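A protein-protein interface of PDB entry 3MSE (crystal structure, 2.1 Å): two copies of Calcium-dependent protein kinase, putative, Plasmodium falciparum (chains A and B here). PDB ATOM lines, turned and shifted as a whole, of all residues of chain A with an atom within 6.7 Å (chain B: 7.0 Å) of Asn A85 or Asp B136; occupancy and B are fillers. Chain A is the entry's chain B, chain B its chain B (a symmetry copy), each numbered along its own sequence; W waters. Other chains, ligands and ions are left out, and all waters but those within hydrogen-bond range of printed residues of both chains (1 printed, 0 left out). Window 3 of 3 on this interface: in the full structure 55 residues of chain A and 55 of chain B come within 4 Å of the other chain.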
ATOM      1  N   ALA A  81      26.173  -7.513 -24.347  1.00  0.00           N
ATOM      2  CA  ALA A  81      26.168  -7.315 -22.892  1.00  0.00           C
ATOM      3  C   ALA A  81      25.011  -6.405 -22.422  1.00  0.00           C
ATOM      4  O   ALA A  81      24.347  -6.687 -21.408  1.00  0.00           O
ATOM      5  CB  ALA A  81      27.508  -6.749 -22.430  1.00  0.00           C
ATOM      6  N   LEU A  82      24.797  -5.317 -23.156  1.00  0.00           N
ATOM      7  CA  LEU A  82      23.723  -4.380 -22.882  1.00  0.00           C
ATOM      8  C   LEU A  82      22.339  -5.021 -23.070  1.00  0.00           C
ATOM      9  O   LEU A  82      21.469  -4.851 -22.217  1.00  0.00           O
ATOM     10  CB  LEU A  82      23.817  -3.156 -23.798  1.00  0.00           C
ATOM     11  CG  LEU A  82      24.947  -2.149 -23.570  1.00  0.00           C
ATOM     12  CD1 LEU A  82      24.738  -0.978 -24.493  1.00  0.00           C
ATOM     13  CD2 LEU A  82      25.020  -1.688 -22.075  1.00  0.00           C
ATOM     14  N   ASP A  83      22.163  -5.743 -24.177  1.00  0.00           N
ATOM     15  CA  ASP A  83      20.876  -6.361 -24.538  1.00  0.00           C
ATOM     16  C   ASP A  83      20.686  -7.625 -23.701  1.00  0.00           C
ATOM     17  O   ASP A  83      20.756  -8.761 -24.188  1.00  0.00           O
ATOM     18  CB  ASP A  83      20.807  -6.668 -26.039  1.00  0.00           C
ATOM     19  CG  ASP A  83      19.363  -6.822 -26.554  1.00  0.00           C
ATOM     20  OD1 ASP A  83      18.405  -6.732 -25.738  1.00  0.00           O
ATOM     21  OD2 ASP A  83      19.195  -7.035 -27.780  1.00  0.00           O
ATOM     22  N   ILE A  84      20.438  -7.393 -22.421  1.00  0.00           N
ATOM     23  CA  ILE A  84      20.434  -8.453 -21.434  1.00  0.00           C
ATOM     24  C   ILE A  84      19.251  -9.407 -21.622  1.00  0.00           C
ATOM     25  O   ILE A  84      19.340 -10.593 -21.280  1.00  0.00           O
ATOM     26  CB  ILE A  84      20.560  -7.834 -20.017  1.00  0.00           C
ATOM     27  CG1 ILE A  84      21.551  -8.623 -19.185  1.00  0.00           C
ATOM     28  CG2 ILE A  84      19.200  -7.530 -19.337  1.00  0.00           C
ATOM     29  CD1 ILE A  84      22.378  -7.729 -18.395  1.00  0.00           C
ATOM     30  N   ASN A  85      18.184  -8.888 -22.232  1.00  0.00           N
ATOM     31  CA  ASN A  85      16.997  -9.670 -22.568  1.00  0.00           C
ATOM     32  C   ASN A  85      16.986 -10.158 -24.014  1.00  0.00           C
ATOM     33  O   ASN A  85      16.015 -10.798 -24.448  1.00  0.00           O
ATOM     34  CB  ASN A  85      15.735  -8.850 -22.269  1.00  0.00           C
ATOM     35  CG  ASN A  85      15.436  -8.775 -20.784  1.00  0.00           C
ATOM     36  OD1 ASN A  85      15.078  -9.779 -20.175  1.00  0.00           O
ATOM     37  ND2 ASN A  85      15.594  -7.593 -20.192  1.00  0.00           N
ATOM     38  N   ASP A  86      18.074  -9.885 -24.740  1.00  0.00           N
ATOM     39  CA  ASP A  86      18.186 -10.219 -26.159  1.00  0.00           C
ATOM     40  C   ASP A  86      16.912  -9.823 -26.920  1.00  0.00           C
ATOM     41  O   ASP A  86      16.324 -10.641 -27.629  1.00  0.00           O
ATOM     42  CB  ASP A  86      18.491 -11.709 -26.341  1.00  0.00           C
ATOM     43  CG  ASP A  86      19.086 -12.028 -27.707  1.00  0.00           C
ATOM     44  OD1 ASP A  86      19.615 -11.103 -28.364  1.00  0.00           O
ATOM     45  OD2 ASP A  86      19.032 -13.211 -28.115  1.00  0.00           O
ATOM     46  N   ARG A  87      16.493  -8.571 -26.752  1.00  0.00           N
ATOM     47  CA  ARG A  87      15.275  -8.064 -27.398  1.00  0.00           C
ATOM     48  C   ARG A  87      15.469  -7.242 -28.681  1.00  0.00           C
ATOM     49  O   ARG A  87      14.482  -6.909 -29.349  1.00  0.00           O
ATOM     50  CB  ARG A  87      14.465  -7.231 -26.397  1.00  0.00           C
ATOM     51  CG  ARG A  87      13.474  -8.023 -25.547  1.00  0.00           C
ATOM     52  CD  ARG A  87      12.427  -7.085 -24.945  1.00  0.00           C
ATOM     53  NE  ARG A  87      13.053  -5.927 -24.299  1.00  0.00           N
ATOM     54  CZ  ARG A  87      13.275  -5.824 -22.991  1.00  0.00           C
ATOM     55  NH1 ARG A  87      12.905  -6.804 -22.166  1.00  0.00           N
ATOM     56  NH2 ARG A  87      13.869  -4.742 -22.503  1.00  0.00           N
ATOM     57  N   GLY A  88      16.711  -6.889 -29.016  1.00  0.00           N
ATOM     58  CA  GLY A  88      16.958  -5.970 -30.136  1.00  0.00           C
ATOM     59  C   GLY A  88      16.573  -4.525 -29.834  1.00  0.00           C
ATOM     60  O   GLY A  88      16.721  -3.640 -30.682  1.00  0.00           O
ATOM     61  N   ASN A  89      16.068  -4.299 -28.623  1.00  0.00           N
ATOM     62  CA  ASN A  89      15.714  -2.984 -28.113  1.00  0.00           C
ATOM     63  C   ASN A  89      16.305  -2.928 -26.707  1.00  0.00           C
ATOM     64  O   ASN A  89      16.120  -3.864 -25.912  1.00  0.00           O
ATOM     65  CB  ASN A  89      14.180  -2.798 -28.063  1.00  0.00           C
ATOM     66  CG  ASN A  89      13.530  -2.845 -29.456  1.00  0.00           C
ATOM     67  OD1 ASN A  89      13.504  -1.839 -30.175  1.00  0.00           O
ATOM     68  ND2 ASN A  89      13.034  -4.016 -29.847  1.00  0.00           N
ATOM     69  N   THR A  91      16.713  -0.915 -23.105  1.00  0.00           N
ATOM     70  CA  THR A  91      16.010   0.072 -22.291  1.00  0.00           C
ATOM     71  C   THR A  91      16.956   1.068 -21.672  1.00  0.00           C
ATOM     72  O   THR A  91      18.177   0.840 -21.612  1.00  0.00           O
ATOM     73  CB  THR A  91      15.194  -0.573 -21.135  1.00  0.00           C
ATOM     74  OG1 THR A  91      16.097  -1.156 -20.201  1.00  0.00           O
ATOM     75  CG2 THR A  91      14.211  -1.633 -21.655  1.00  0.00           C
ATOM     76  N   GLU A  94      18.822  -0.640 -18.876  1.00  0.00           N
ATOM     77  CA  GLU A  94      19.879  -1.515 -19.405  1.00  0.00           C
ATOM     78  C   GLU A  94      21.108  -0.755 -19.944  1.00  0.00           C
ATOM     79  O   GLU A  94      22.255  -1.215 -19.771  1.00  0.00           O
ATOM     80  CB  GLU A  94      19.305  -2.455 -20.450  1.00  0.00           C
ATOM     81  CG  GLU A  94      18.226  -3.390 -19.843  1.00  0.00           C
ATOM     82  CD  GLU A  94      17.322  -4.036 -20.887  1.00  0.00           C
ATOM     83  OE1 GLU A  94      16.432  -4.816 -20.475  1.00  0.00           O
ATOM     84  OE2 GLU A  94      17.495  -3.790 -22.109  1.00  0.00           O
ATOM     85  N   ILE B  22      22.943  -8.935 -14.999  1.00  0.00           N
ATOM     86  CA  ILE B  22      21.541  -8.946 -14.546  1.00  0.00           C
ATOM     87  C   ILE B  22      21.443  -8.348 -13.139  1.00  0.00           C
ATOM     88  O   ILE B  22      20.607  -7.469 -12.882  1.00  0.00           O
ATOM     89  CB  ILE B  22      20.933 -10.350 -14.642  1.00  0.00           C
ATOM     90  CG1 ILE B  22      20.689 -10.664 -16.118  1.00  0.00           C
ATOM     91  CG2 ILE B  22      19.575 -10.418 -13.850  1.00  0.00           C
ATOM     92  CD1 ILE B  22      20.558 -12.126 -16.424  1.00  0.00           C
ATOM     93  N   ASN B  25      21.837  -4.744 -13.298  1.00  0.00           N
ATOM     94  CA  ASN B  25      20.546  -4.115 -13.690  1.00  0.00           C
ATOM     95  C   ASN B  25      19.546  -3.876 -12.533  1.00  0.00           C
ATOM     96  O   ASN B  25      18.828  -2.874 -12.531  1.00  0.00           O
ATOM     97  CB  ASN B  25      19.858  -4.888 -14.822  1.00  0.00           C
ATOM     98  CG  ASN B  25      20.279  -4.400 -16.195  1.00  0.00           C
ATOM     99  OD1 ASN B  25      19.566  -3.626 -16.828  1.00  0.00           O
ATOM    100  ND2 ASN B  25      21.453  -4.848 -16.659  1.00  0.00           N
ATOM    101  N   VAL B 131      17.951 -19.461 -10.655  1.00  0.00           N
ATOM    102  CA  VAL B 131      17.036 -19.980 -11.677  1.00  0.00           C
ATOM    103  C   VAL B 131      15.852 -19.016 -11.821  1.00  0.00           C
ATOM    104  O   VAL B 131      15.422 -18.678 -12.935  1.00  0.00           O
ATOM    105  CB  VAL B 131      16.560 -21.422 -11.343  1.00  0.00           C
ATOM    106  CG1 VAL B 131      15.466 -21.906 -12.333  1.00  0.00           C
ATOM    107  CG2 VAL B 131      17.739 -22.401 -11.330  1.00  0.00           C
ATOM    108  N   SER B 132      15.357 -18.528 -10.693  1.00  0.00           N
ATOM    109  CA  SER B 132      14.213 -17.637 -10.732  1.00  0.00           C
ATOM    110  C   SER B 132      14.594 -16.280 -11.317  1.00  0.00           C
ATOM    111  O   SER B 132      13.879 -15.721 -12.162  1.00  0.00           O
ATOM    112  CB  SER B 132      13.611 -17.475  -9.331  1.00  0.00           C
ATOM    113  OG  SER B 132      12.540 -16.553  -9.408  1.00  0.00           O
ATOM    114  N   LEU B 133      15.736 -15.766 -10.872  1.00  0.00           N
ATOM    115  CA  LEU B 133      16.259 -14.502 -11.378  1.00  0.00           C
ATOM    116  C   LEU B 133      16.343 -14.504 -12.913  1.00  0.00           C
ATOM    117  O   LEU B 133      16.064 -13.498 -13.551  1.00  0.00           O
ATOM    118  CB  LEU B 133      17.647 -14.204 -10.757  1.00  0.00           C
ATOM    119  CG  LEU B 133      18.304 -12.881 -11.159  1.00  0.00           C
ATOM    120  CD1 LEU B 133      17.476 -11.696 -10.685  1.00  0.00           C
ATOM    121  CD2 LEU B 133      19.704 -12.789 -10.587  1.00  0.00           C
ATOM    122  N   VAL B 134      16.685 -15.643 -13.503  1.00  0.00           N
ATOM    123  CA  VAL B 134      16.857 -15.690 -14.949  1.00  0.00           C
ATOM    124  C   VAL B 134      15.664 -16.268 -15.689  1.00  0.00           C
ATOM    125  O   VAL B 134      15.778 -16.674 -16.864  1.00  0.00           O
ATOM    126  CB  VAL B 134      18.183 -16.403 -15.344  1.00  0.00           C
ATOM    127  CG1 VAL B 134      19.354 -15.715 -14.640  1.00  0.00           C
ATOM    128  CG2 VAL B 134      18.146 -17.890 -14.993  1.00  0.00           C
ATOM    129  N   HIS B 135      14.514 -16.279 -15.018  1.00  0.00           N
ATOM    130  CA  HIS B 135      13.299 -16.919 -15.560  1.00  0.00           C
ATOM    131  C   HIS B 135      12.845 -16.282 -16.886  1.00  0.00           C
ATOM    132  O   HIS B 135      12.212 -16.938 -17.711  1.00  0.00           O
ATOM    133  CB  HIS B 135      12.155 -16.865 -14.522  1.00  0.00           C
ATOM    134  CG  HIS B 135      11.453 -15.548 -14.497  1.00  0.00           C
ATOM    135  ND1 HIS B 135      12.011 -14.421 -13.935  1.00  0.00           N
ATOM    136  CD2 HIS B 135      10.276 -15.158 -15.033  1.00  0.00           C
ATOM    137  CE1 HIS B 135      11.194 -13.398 -14.108  1.00  0.00           C
ATOM    138  NE2 HIS B 135      10.130 -13.820 -14.769  1.00  0.00           N
ATOM    139  N   ASP B 136      13.172 -15.005 -17.095  1.00  0.00           N
ATOM    140  CA  ASP B 136      12.810 -14.342 -18.349  1.00  0.00           C
ATOM    141  C   ASP B 136      14.000 -14.161 -19.310  1.00  0.00           C
ATOM    142  O   ASP B 136      13.985 -13.279 -20.162  1.00  0.00           O
ATOM    143  CB  ASP B 136      12.126 -12.990 -18.078  1.00  0.00           C
ATOM    144  CG  ASP B 136      13.022 -12.000 -17.305  1.00  0.00           C
ATOM    145  OD1 ASP B 136      12.532 -10.886 -17.040  1.00  0.00           O
ATOM    146  OD2 ASP B 136      14.187 -12.313 -16.943  1.00  0.00           O
ATOM    147  N   LYS B 137      15.021 -14.993 -19.152  1.00  0.00           N
ATOM    148  CA  LYS B 137      16.245 -14.897 -19.947  1.00  0.00           C
ATOM    149  C   LYS B 137      16.528 -16.262 -20.512  1.00  0.00           C
ATOM    150  O   LYS B 137      16.243 -17.284 -19.868  1.00  0.00           O
ATOM    151  CB  LYS B 137      17.444 -14.470 -19.074  1.00  0.00           C
ATOM    152  CG  LYS B 137      17.242 -13.236 -18.209  1.00  0.00           C
ATOM    153  CD  LYS B 137      17.295 -11.958 -19.030  1.00  0.00           C
ATOM    154  CE  LYS B 137      17.357 -10.711 -18.137  1.00  0.00           C
ATOM    155  NZ  LYS B 137      16.027 -10.338 -17.560  1.00  0.00           N
ATOM    156  N   VAL B 138      17.099 -16.283 -21.711  1.00  0.00           N
ATOM    157  CA  VAL B 138      17.356 -17.536 -22.431  1.00  0.00           C
ATOM    158  C   VAL B 138      18.446 -18.415 -21.780  1.00  0.00           C
ATOM    159  O   VAL B 138      18.605 -19.586 -22.149  1.00  0.00           O
ATOM    160  CB  VAL B 138      17.592 -17.281 -23.959  1.00  0.00           C
ATOM    161  CG1 VAL B 138      18.652 -16.189 -24.188  1.00  0.00           C
ATOM    162  CG2 VAL B 138      17.958 -18.562 -24.695  1.00  0.00           C
ATOM    163  N   LEU B 139      19.154 -17.869 -20.792  1.00  0.00           N
ATOM    164  CA  LEU B 139      20.176 -18.596 -20.013  1.00  0.00           C
ATOM    165  C   LEU B 139      19.695 -19.927 -19.425  1.00  0.00           C
ATOM    166  O   LEU B 139      18.507 -20.092 -19.135  1.00  0.00           O
ATOM    167  CB  LEU B 139      20.704 -17.728 -18.862  1.00  0.00           C
ATOM    168  CG  LEU B 139      21.073 -16.267 -19.106  1.00  0.00           C
ATOM    169  CD1 LEU B 139      21.314 -15.593 -17.766  1.00  0.00           C
ATOM    170  CD2 LEU B 139      22.302 -16.151 -20.000  1.00  0.00           C
HETATM  171  O   HOH W   1      22.342  -3.808 -19.554  1.00  0.00           O
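The side-chain amide oxygen of Asn A85 lies within hydrogen-bond range of the side-chain amino group of Lys B137, at 2.8 Å.
The side-chain hydroxyl of Thr A91 sits at hydrogen-bond distance from the backbone NH of Glu A94, at 3.1 Å. NH2 of Arg A87 lies within salt-bridge range of OE1 of Glu A94 (3.3 Å). ND2 of Asn A85 lies close to NH1 of Arg A87, at 3.4 Å. The side-chain carboxylate (OD2) of Asp B136 lies within salt-bridge range of the side-chain amino group (NZ) of Lys B137, 2.8 Å away. The side-chain carboxylate (OE1) of Glu A94 sits at hydrogen-bond distance from the side-chain amide nitrogen (ND2) of Asn A85.
N of Ile B22 touches CD1 of Ile A84, 3.6 Å away. Ile A84 touches Asn B25 (CD1 to ND2, 3.5 Å). O of Ile A84 touches CD of Lys B137 (3.3 Å). OD1 of Asn A85 touches O of Asp B136, at 3.7 Å. Glu A94 touches Asn B25.
Asn A85 touches just these residues of chain B: Asp B136 and Lys B137. Asp B136 touches one residue of chain A. Of the printed residues of chain B, Glu A94 touches Asn B25 (3.3 Å). Printed residues of chain A within 4 Å of Asn B25: Ile A84 (3.5 Å) and Glu A94 (3.3 Å). Asp A86 touches none of the printed residues of chain B. The nearest residue of chain A that does not touch Asp B136 is Ile A84 (6.1 Å). The nearest printed residue of chain B that does not touch Ile A84 is Asp B136 (6.1 Å).
Of the 11 printed residues of chain A, 3 touch a printed residue of chain B.
No position is printed for both chains. Of the 6 pairs that touch across the chains among the printed residues, none has its exchanged pair printed and touching as well.
Water W1 lies within hydrogen-bond range of the backbone carbonyl oxygen of Glu A94 (2.6 Å), the backbone carbonyl oxygen of Leu A82 (3.0 Å) and the side-chain amide nitrogen of Asn B25 (3.2 Å).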
